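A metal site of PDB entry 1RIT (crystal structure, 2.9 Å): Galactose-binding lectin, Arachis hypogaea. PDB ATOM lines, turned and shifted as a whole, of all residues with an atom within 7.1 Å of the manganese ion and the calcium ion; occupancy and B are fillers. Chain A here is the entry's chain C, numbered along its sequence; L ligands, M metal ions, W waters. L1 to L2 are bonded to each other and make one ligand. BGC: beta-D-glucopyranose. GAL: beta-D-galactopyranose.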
ATOM      1  N   ALA A  82     -25.062 -21.070   4.965  1.00  0.00           N
ATOM      2  CA  ALA A  82     -23.811 -20.337   4.777  1.00  0.00           C
ATOM      3  C   ALA A  82     -23.267 -19.852   6.129  1.00  0.00           C
ATOM      4  O   ALA A  82     -24.019 -19.788   7.101  1.00  0.00           O
ATOM      5  CB  ALA A  82     -24.049 -19.158   3.829  1.00  0.00           C
ATOM      6  N   ASP A  83     -21.968 -19.530   6.198  1.00  0.00           N
ATOM      7  CA  ASP A  83     -21.041 -19.601   5.063  1.00  0.00           C
ATOM      8  C   ASP A  83     -20.042 -20.771   5.063  1.00  0.00           C
ATOM      9  O   ASP A  83     -19.493 -21.127   4.020  1.00  0.00           O
ATOM     10  CB  ASP A  83     -20.247 -18.292   4.963  1.00  0.00           C
ATOM     11  CG  ASP A  83     -21.086 -17.142   4.496  1.00  0.00           C
ATOM     12  OD1 ASP A  83     -20.872 -16.697   3.349  1.00  0.00           O
ATOM     13  OD2 ASP A  83     -21.969 -16.693   5.260  1.00  0.00           O
ATOM     14  N   GLY A  84     -19.805 -21.349   6.225  1.00  0.00           N
ATOM     15  CA  GLY A  84     -18.866 -22.454   6.303  1.00  0.00           C
ATOM     16  C   GLY A  84     -17.905 -22.341   7.475  1.00  0.00           C
ATOM     17  O   GLY A  84     -18.000 -21.448   8.319  1.00  0.00           O
ATOM     18  N   GLY A 103     -20.155 -13.337   7.028  1.00  0.00           N
ATOM     19  CA  GLY A 103     -20.363 -14.092   5.802  1.00  0.00           C
ATOM     20  C   GLY A 103     -19.154 -14.647   5.080  1.00  0.00           C
ATOM     21  O   GLY A 103     -18.340 -15.367   5.652  1.00  0.00           O
ATOM     22  N   GLY A 104     -19.051 -14.293   3.805  1.00  0.00           N
ATOM     23  CA  GLY A 104     -17.952 -14.755   2.969  1.00  0.00           C
ATOM     24  C   GLY A 104     -16.525 -14.547   3.454  1.00  0.00           C
ATOM     25  O   GLY A 104     -15.601 -15.121   2.864  1.00  0.00           O
ATOM     26  N   THR A 105     -16.320 -13.741   4.499  1.00  0.00           N
ATOM     27  CA  THR A 105     -14.968 -13.503   5.004  1.00  0.00           C
ATOM     28  C   THR A 105     -14.575 -14.588   6.006  1.00  0.00           C
ATOM     29  O   THR A 105     -13.423 -14.664   6.421  1.00  0.00           O
ATOM     30  CB  THR A 105     -14.819 -12.127   5.689  1.00  0.00           C
ATOM     31  OG1 THR A 105     -15.616 -12.072   6.874  1.00  0.00           O
ATOM     32  CG2 THR A 105     -15.262 -11.032   4.757  1.00  0.00           C
ATOM     33  N   LEU A 106     -15.557 -15.412   6.364  1.00  0.00           N
ATOM     34  CA  LEU A 106     -15.355 -16.523   7.301  1.00  0.00           C
ATOM     35  C   LEU A 106     -14.787 -16.124   8.660  1.00  0.00           C
ATOM     36  O   LEU A 106     -14.413 -16.982   9.447  1.00  0.00           O
ATOM     37  CB  LEU A 106     -14.459 -17.599   6.672  1.00  0.00           C
ATOM     38  CG  LEU A 106     -15.031 -18.310   5.439  1.00  0.00           C
ATOM     39  CD1 LEU A 106     -13.982 -19.257   4.868  1.00  0.00           C
ATOM     40  CD2 LEU A 106     -16.310 -19.057   5.826  1.00  0.00           C
ATOM     41  N   GLU A 121     -10.423 -24.025   4.411  1.00  0.00           N
ATOM     42  CA  GLU A 121     -11.834 -23.712   4.523  1.00  0.00           C
ATOM     43  C   GLU A 121     -12.744 -24.782   3.932  1.00  0.00           C
ATOM     44  O   GLU A 121     -12.392 -25.443   2.953  1.00  0.00           O
ATOM     45  CB  GLU A 121     -12.119 -22.395   3.823  1.00  0.00           C
ATOM     46  CG  GLU A 121     -11.746 -22.423   2.347  1.00  0.00           C
ATOM     47  CD  GLU A 121     -12.287 -21.254   1.563  1.00  0.00           C
ATOM     48  OE1 GLU A 121     -11.822 -20.111   1.782  1.00  0.00           O
ATOM     49  OE2 GLU A 121     -13.198 -21.490   0.740  1.00  0.00           O
ATOM     50  N   PHE A 122     -13.898 -24.930   4.555  1.00  0.00           N
ATOM     51  CA  PHE A 122     -14.929 -25.862   4.113  1.00  0.00           C
ATOM     52  C   PHE A 122     -16.086 -24.920   3.810  1.00  0.00           C
ATOM     53  O   PHE A 122     -17.032 -24.788   4.586  1.00  0.00           O
ATOM     54  CB  PHE A 122     -15.243 -26.849   5.233  1.00  0.00           C
ATOM     55  CG  PHE A 122     -14.064 -27.711   5.633  1.00  0.00           C
ATOM     56  CD1 PHE A 122     -13.019 -27.178   6.381  1.00  0.00           C
ATOM     57  CD2 PHE A 122     -13.957 -29.035   5.187  1.00  0.00           C
ATOM     58  CE1 PHE A 122     -11.888 -27.958   6.676  1.00  0.00           C
ATOM     59  CE2 PHE A 122     -12.833 -29.803   5.479  1.00  0.00           C
ATOM     60  CZ  PHE A 122     -11.802 -29.271   6.224  1.00  0.00           C
ATOM     61  N   ASP A 123     -15.935 -24.267   2.652  1.00  0.00           N
ATOM     62  CA  ASP A 123     -16.842 -23.278   2.079  1.00  0.00           C
ATOM     63  C   ASP A 123     -18.185 -23.859   1.584  1.00  0.00           C
ATOM     64  O   ASP A 123     -18.192 -24.860   0.863  1.00  0.00           O
ATOM     65  CB  ASP A 123     -16.085 -22.598   0.903  1.00  0.00           C
ATOM     66  CG  ASP A 123     -16.531 -21.155   0.656  1.00  0.00           C
ATOM     67  OD1 ASP A 123     -17.726 -20.879   0.887  1.00  0.00           O
ATOM     68  OD2 ASP A 123     -15.706 -20.296   0.223  1.00  0.00           O
ATOM     69  N   THR A 124     -19.308 -23.234   1.963  1.00  0.00           N
ATOM     70  CA  THR A 124     -20.631 -23.708   1.521  1.00  0.00           C
ATOM     71  C   THR A 124     -21.448 -22.657   0.758  1.00  0.00           C
ATOM     72  O   THR A 124     -22.647 -22.861   0.521  1.00  0.00           O
ATOM     73  CB  THR A 124     -21.529 -24.202   2.688  1.00  0.00           C
ATOM     74  OG1 THR A 124     -21.872 -23.086   3.517  1.00  0.00           O
ATOM     75  CG2 THR A 124     -20.858 -25.310   3.495  1.00  0.00           C
ATOM     76  N   TYR A 125     -20.832 -21.541   0.397  1.00  0.00           N
ATOM     77  CA  TYR A 125     -21.534 -20.508  -0.372  1.00  0.00           C
ATOM     78  C   TYR A 125     -20.569 -19.854  -1.354  1.00  0.00           C
ATOM     79  O   TYR A 125     -19.437 -19.518  -1.008  1.00  0.00           O
ATOM     80  CB  TYR A 125     -22.120 -19.428   0.540  1.00  0.00           C
ATOM     81  CG  TYR A 125     -22.886 -18.374  -0.230  1.00  0.00           C
ATOM     82  CD1 TYR A 125     -24.254 -18.500  -0.441  1.00  0.00           C
ATOM     83  CD2 TYR A 125     -22.234 -17.263  -0.777  1.00  0.00           C
ATOM     84  CE1 TYR A 125     -24.963 -17.557  -1.182  1.00  0.00           C
ATOM     85  CE2 TYR A 125     -22.931 -16.308  -1.508  1.00  0.00           C
ATOM     86  CZ  TYR A 125     -24.291 -16.463  -1.716  1.00  0.00           C
ATOM     87  OH  TYR A 125     -24.988 -15.516  -2.439  1.00  0.00           O
ATOM     88  N   SER A 126     -21.014 -19.656  -2.584  1.00  0.00           N
ATOM     89  CA  SER A 126     -20.125 -19.074  -3.569  1.00  0.00           C
ATOM     90  C   SER A 126     -20.145 -17.535  -3.526  1.00  0.00           C
ATOM     91  O   SER A 126     -21.191 -16.908  -3.707  1.00  0.00           O
ATOM     92  CB  SER A 126     -20.516 -19.572  -4.960  1.00  0.00           C
ATOM     93  OG  SER A 126     -19.498 -19.307  -5.916  1.00  0.00           O
ATOM     94  N   ASN A 127     -18.983 -16.959  -3.261  1.00  0.00           N
ATOM     95  CA  ASN A 127     -18.816 -15.500  -3.205  1.00  0.00           C
ATOM     96  C   ASN A 127     -18.030 -15.069  -4.434  1.00  0.00           C
ATOM     97  O   ASN A 127     -16.802 -15.149  -4.440  1.00  0.00           O
ATOM     98  CB  ASN A 127     -18.037 -15.094  -1.954  1.00  0.00           C
ATOM     99  CG  ASN A 127     -18.851 -15.246  -0.684  1.00  0.00           C
ATOM    100  OD1 ASN A 127     -19.382 -16.317  -0.395  1.00  0.00           O
ATOM    101  ND2 ASN A 127     -18.959 -14.168   0.094  1.00  0.00           N
ATOM    102  N   TYR A 130     -14.880 -13.158  -4.253  1.00  0.00           N
ATOM    103  CA  TYR A 130     -13.671 -13.803  -3.742  1.00  0.00           C
ATOM    104  C   TYR A 130     -13.202 -14.903  -4.680  1.00  0.00           C
ATOM    105  O   TYR A 130     -12.332 -15.705  -4.333  1.00  0.00           O
ATOM    106  CB  TYR A 130     -13.916 -14.366  -2.342  1.00  0.00           C
ATOM    107  CG  TYR A 130     -14.314 -13.323  -1.315  1.00  0.00           C
ATOM    108  CD1 TYR A 130     -13.500 -12.206  -1.089  1.00  0.00           C
ATOM    109  CD2 TYR A 130     -15.490 -13.453  -0.573  1.00  0.00           C
ATOM    110  CE1 TYR A 130     -13.864 -11.234  -0.160  1.00  0.00           C
ATOM    111  CE2 TYR A 130     -15.862 -12.482   0.368  1.00  0.00           C
ATOM    112  CZ  TYR A 130     -15.037 -11.368   0.565  1.00  0.00           C
ATOM    113  OH  TYR A 130     -15.391 -10.405   1.474  1.00  0.00           O
ATOM    114  N   ASN A 131     -13.785 -14.927  -5.889  1.00  0.00           N
ATOM    115  CA  ASN A 131     -13.459 -15.921  -6.919  1.00  0.00           C
ATOM    116  C   ASN A 131     -13.850 -17.333  -6.516  1.00  0.00           C
ATOM    117  O   ASN A 131     -13.228 -18.299  -6.955  1.00  0.00           O
ATOM    118  CB  ASN A 131     -11.963 -15.908  -7.245  1.00  0.00           C
ATOM    119  CG  ASN A 131     -11.556 -14.738  -8.107  1.00  0.00           C
ATOM    120  OD1 ASN A 131     -12.209 -14.425  -9.097  1.00  0.00           O
ATOM    121  ND2 ASN A 131     -10.458 -14.081  -7.738  1.00  0.00           N
ATOM    122  N   ASP A 132     -14.885 -17.447  -5.695  1.00  0.00           N
ATOM    123  CA  ASP A 132     -15.379 -18.747  -5.231  1.00  0.00           C
ATOM    124  C   ASP A 132     -15.841 -19.654  -6.372  1.00  0.00           C
ATOM    125  O   ASP A 132     -16.453 -19.186  -7.330  1.00  0.00           O
ATOM    126  CB  ASP A 132     -16.555 -18.562  -4.257  1.00  0.00           C
ATOM    127  CG  ASP A 132     -16.189 -18.872  -2.799  1.00  0.00           C
ATOM    128  OD1 ASP A 132     -15.010 -19.193  -2.553  1.00  0.00           O
ATOM    129  OD2 ASP A 132     -17.081 -18.801  -1.911  1.00  0.00           O
ATOM    130  N   PRO A 133     -15.521 -20.958  -6.307  1.00  0.00           N
ATOM    131  CA  PRO A 133     -15.950 -21.884  -7.355  1.00  0.00           C
ATOM    132  C   PRO A 133     -17.485 -21.967  -7.225  1.00  0.00           C
ATOM    133  O   PRO A 133     -18.042 -21.731  -6.141  1.00  0.00           O
ATOM    134  CB  PRO A 133     -15.261 -23.184  -6.964  1.00  0.00           C
ATOM    135  CG  PRO A 133     -13.975 -22.701  -6.319  1.00  0.00           C
ATOM    136  CD  PRO A 133     -14.487 -21.579  -5.445  1.00  0.00           C
ATOM    137  N   HIS A 137     -16.977 -26.357  -1.666  1.00  0.00           N
ATOM    138  CA  HIS A 137     -15.610 -26.732  -1.941  1.00  0.00           C
ATOM    139  C   HIS A 137     -14.770 -26.690  -0.682  1.00  0.00           C
ATOM    140  O   HIS A 137     -15.204 -26.238   0.387  1.00  0.00           O
ATOM    141  CB  HIS A 137     -15.024 -25.797  -2.991  1.00  0.00           C
ATOM    142  CG  HIS A 137     -15.202 -24.345  -2.651  1.00  0.00           C
ATOM    143  ND1 HIS A 137     -16.440 -23.743  -2.580  1.00  0.00           N
ATOM    144  CD2 HIS A 137     -14.298 -23.382  -2.352  1.00  0.00           C
ATOM    145  CE1 HIS A 137     -16.290 -22.473  -2.251  1.00  0.00           C
ATOM    146  NE2 HIS A 137     -15.005 -22.228  -2.103  1.00  0.00           N
ATOM    147  N   VAL A 138     -13.542 -27.175  -0.826  1.00  0.00           N
ATOM    148  CA  VAL A 138     -12.603 -27.195   0.269  1.00  0.00           C
ATOM    149  C   VAL A 138     -11.438 -26.412  -0.320  1.00  0.00           C
ATOM    150  O   VAL A 138     -11.128 -26.567  -1.515  1.00  0.00           O
ATOM    151  CB  VAL A 138     -12.190 -28.643   0.615  1.00  0.00           C
ATOM    152  CG1 VAL A 138     -11.209 -28.650   1.778  1.00  0.00           C
ATOM    153  CG2 VAL A 138     -13.440 -29.471   0.960  1.00  0.00           C
ATOM    154  N   GLY A 139     -10.800 -25.570   0.474  1.00  0.00           N
ATOM    155  CA  GLY A 139      -9.695 -24.811  -0.074  1.00  0.00           C
ATOM    156  C   GLY A 139      -8.534 -24.503   0.845  1.00  0.00           C
ATOM    157  O   GLY A 139      -8.650 -24.535   2.080  1.00  0.00           O
ATOM    158  N   ASP A 141      -6.195 -21.662   1.895  1.00  0.00           N
ATOM    159  CA  ASP A 141      -6.142 -20.215   1.892  1.00  0.00           C
ATOM    160  C   ASP A 141      -4.837 -19.726   2.490  1.00  0.00           C
ATOM    161  O   ASP A 141      -4.369 -20.269   3.491  1.00  0.00           O
ATOM    162  CB  ASP A 141      -7.332 -19.666   2.690  1.00  0.00           C
ATOM    163  CG  ASP A 141      -8.665 -20.184   2.157  1.00  0.00           C
ATOM    164  OD1 ASP A 141      -8.704 -20.630   0.987  1.00  0.00           O
ATOM    165  OD2 ASP A 141      -9.675 -20.145   2.900  1.00  0.00           O
ATOM    166  N   VAL A 145      -9.123 -15.169   1.486  1.00  0.00           N
ATOM    167  CA  VAL A 145     -10.182 -16.162   1.254  1.00  0.00           C
ATOM    168  C   VAL A 145     -10.330 -16.411  -0.271  1.00  0.00           C
ATOM    169  O   VAL A 145     -11.277 -17.078  -0.716  1.00  0.00           O
ATOM    170  CB  VAL A 145     -11.540 -15.714   1.871  1.00  0.00           C
ATOM    171  CG1 VAL A 145     -11.459 -15.768   3.381  1.00  0.00           C
ATOM    172  CG2 VAL A 145     -11.911 -14.306   1.402  1.00  0.00           C
ATOM    173  N   ASP A 146      -9.399 -15.858  -1.053  1.00  0.00           N
ATOM    174  CA  ASP A 146      -9.365 -16.066  -2.501  1.00  0.00           C
ATOM    175  C   ASP A 146      -8.353 -17.189  -2.565  1.00  0.00           C
ATOM    176  O   ASP A 146      -7.166 -16.982  -2.804  1.00  0.00           O
ATOM    177  CB  ASP A 146      -8.811 -14.832  -3.229  1.00  0.00           C
ATOM    178  CG  ASP A 146      -8.835 -14.977  -4.747  1.00  0.00           C
ATOM    179  OD1 ASP A 146      -8.162 -15.898  -5.274  1.00  0.00           O
ATOM    180  OD2 ASP A 146      -9.520 -14.174  -5.408  1.00  0.00           O
ATOM    181  N   SER A 147      -8.866 -18.379  -2.287  1.00  0.00           N
ATOM    182  CA  SER A 147      -8.070 -19.597  -2.239  1.00  0.00           C
ATOM    183  C   SER A 147      -6.959 -19.739  -3.275  1.00  0.00           C
ATOM    184  O   SER A 147      -7.125 -19.383  -4.438  1.00  0.00           O
ATOM    185  CB  SER A 147      -9.004 -20.808  -2.318  1.00  0.00           C
ATOM    186  OG  SER A 147     -10.100 -20.666  -1.413  1.00  0.00           O
ATOM    187  N   THR A 150      -8.590 -24.895  -4.636  1.00  0.00           N
ATOM    188  CA  THR A 150      -9.800 -25.485  -4.083  1.00  0.00           C
ATOM    189  C   THR A 150     -10.042 -26.818  -4.779  1.00  0.00           C
ATOM    190  O   THR A 150      -9.386 -27.152  -5.767  1.00  0.00           O
ATOM    191  CB  THR A 150     -11.065 -24.597  -4.296  1.00  0.00           C
ATOM    192  OG1 THR A 150     -11.341 -24.451  -5.690  1.00  0.00           O
ATOM    193  CG2 THR A 150     -10.866 -23.235  -3.672  1.00  0.00           C
HETATM  194  C2  BGC L   1     -28.464 -10.379   1.734  1.00  0.00           C
HETATM  195  C3  BGC L   1     -27.083 -10.826   2.246  1.00  0.00           C
HETATM  196  C4  BGC L   1     -26.150 -11.028   1.037  1.00  0.00           C
HETATM  197  C5  BGC L   1     -26.047  -9.679   0.238  1.00  0.00           C
HETATM  198  C6  BGC L   1     -25.171  -9.782  -1.009  1.00  0.00           C
HETATM  199  C1  BGC L   1     -28.311  -9.064   0.950  1.00  0.00           C
HETATM  200  O1  BGC L   1     -29.532  -8.637   0.474  1.00  0.00           O
HETATM  201  O2  BGC L   1     -29.341 -10.187   2.833  1.00  0.00           O
HETATM  202  O3  BGC L   1     -27.182 -12.040   2.976  1.00  0.00           O
HETATM  203  O4  BGC L   1     -24.841 -11.461   1.488  1.00  0.00           O
HETATM  204  O5  BGC L   1     -27.395  -9.228  -0.187  1.00  0.00           O
HETATM  205  O6  BGC L   1     -25.437 -10.959  -1.783  1.00  0.00           O
HETATM  206  C1  GAL L   2     -24.422 -12.760   1.169  1.00  0.00           C
HETATM  207  C2  GAL L   2     -23.013 -12.979   1.747  1.00  0.00           C
HETATM  208  C3  GAL L   2     -22.517 -14.390   1.417  1.00  0.00           C
HETATM  209  C4  GAL L   2     -23.496 -15.444   2.013  1.00  0.00           C
HETATM  210  C5  GAL L   2     -24.881 -15.132   1.384  1.00  0.00           C
HETATM  211  C6  GAL L   2     -26.015 -16.001   1.783  1.00  0.00           C
HETATM  212  O2  GAL L   2     -22.123 -12.010   1.216  1.00  0.00           O
HETATM  213  O3  GAL L   2     -21.218 -14.563   1.946  1.00  0.00           O
HETATM  214  O4  GAL L   2     -23.547 -15.281   3.434  1.00  0.00           O
HETATM  215  O5  GAL L   2     -25.282 -13.769   1.708  1.00  0.00           O
HETATM  216  O6  GAL L   2     -27.106 -15.781   0.902  1.00  0.00           O
HETATM  217 MN    MN M   1     -13.711 -20.409  -0.899  1.00  0.00          MN
HETATM  218 CA    CA M   2     -18.039 -18.395   0.928  1.00  0.00          CA
HETATM  219  O   HOH W   1     -12.159 -19.100  -2.233  1.00  0.00           O
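The calcium ion is bound by OD1 of Asp 123, O of Tyr 125 and OD1 of Asn 127.
Slightly farther from the calcium ion lies the side-chain carboxylate (OD2) of Asp 132 (3.0 Å).
Slightly farther from the calcium ion lies the side-chain carboxylate (OD2) of Asp 123 (3.1 Å).
OG of Ser 147 touches the manganese ion (3.7 Å).
Of the 26 residues printed, 5 come within 4 Å of the manganese ion.
Along chain A the residues within 4 Å of the manganese ion span positions 121 to 147.
Within 4 Å of the calcium ion: Asp 123, Tyr 125, Asn 127 and Asp 132.
The nearest printed residue that does not touch the calcium ion is Asp 83 (4.1 Å).
The manganese ion is bound by OE2 of Glu 121, at 2.0 Å.
The manganese ion is bound by OD2 of Asp 123, at 2.3 Å.
Water W1 binds the manganese ion (2.4 Å).
The manganese ion is bound by OD1 of Asp 132 (2.4 Å).
The manganese ion is bound by NE2 of His 137, 2.5 Å away.
The manganese ion has five donor atoms within binding distance.
Water W1 bridges O of Val 145 and OG of Ser 147.
The side-chain carboxylate of Asp 141 lies within hydrogen-bond range of the side-chain hydroxyl of Ser 147, 2.8 Å away.
The backbone carbonyl oxygen of Glu 121 is in hydrogen-bond range of the backbone NH of Gly 139 (2.9 Å).
The side-chain carboxylate (OD2) of Asp 132 sits close to the backbone carbonyl oxygen (O) of Tyr 125, at 2.6 Å.
OD2 of Asp 132 lies within hydrogen-bond range of N of Asn 127, 3.0 Å away.
The side-chain carboxylate (OD2) of Asp 141 lies close to the side-chain carboxylate (OE1) of Glu 121 (2.4 Å).
The side-chain hydroxyl (OG) of Ser 126 sits at hydrogen-bond distance from the backbone carbonyl oxygen (O) of Asp 132, 3.4 Å away.
OD1 of Asp 83 sits at hydrogen-bond distance from O3 of GAL L2 (2.6 Å).
An oxygen (O3) of GAL L2 lies within hydrogen-bond range of the backbone NH of Gly 104, 2.9 Å away.
ND2 of Asn 127 sits at hydrogen-bond distance from O3 of GAL L2, 2.9 Å away.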
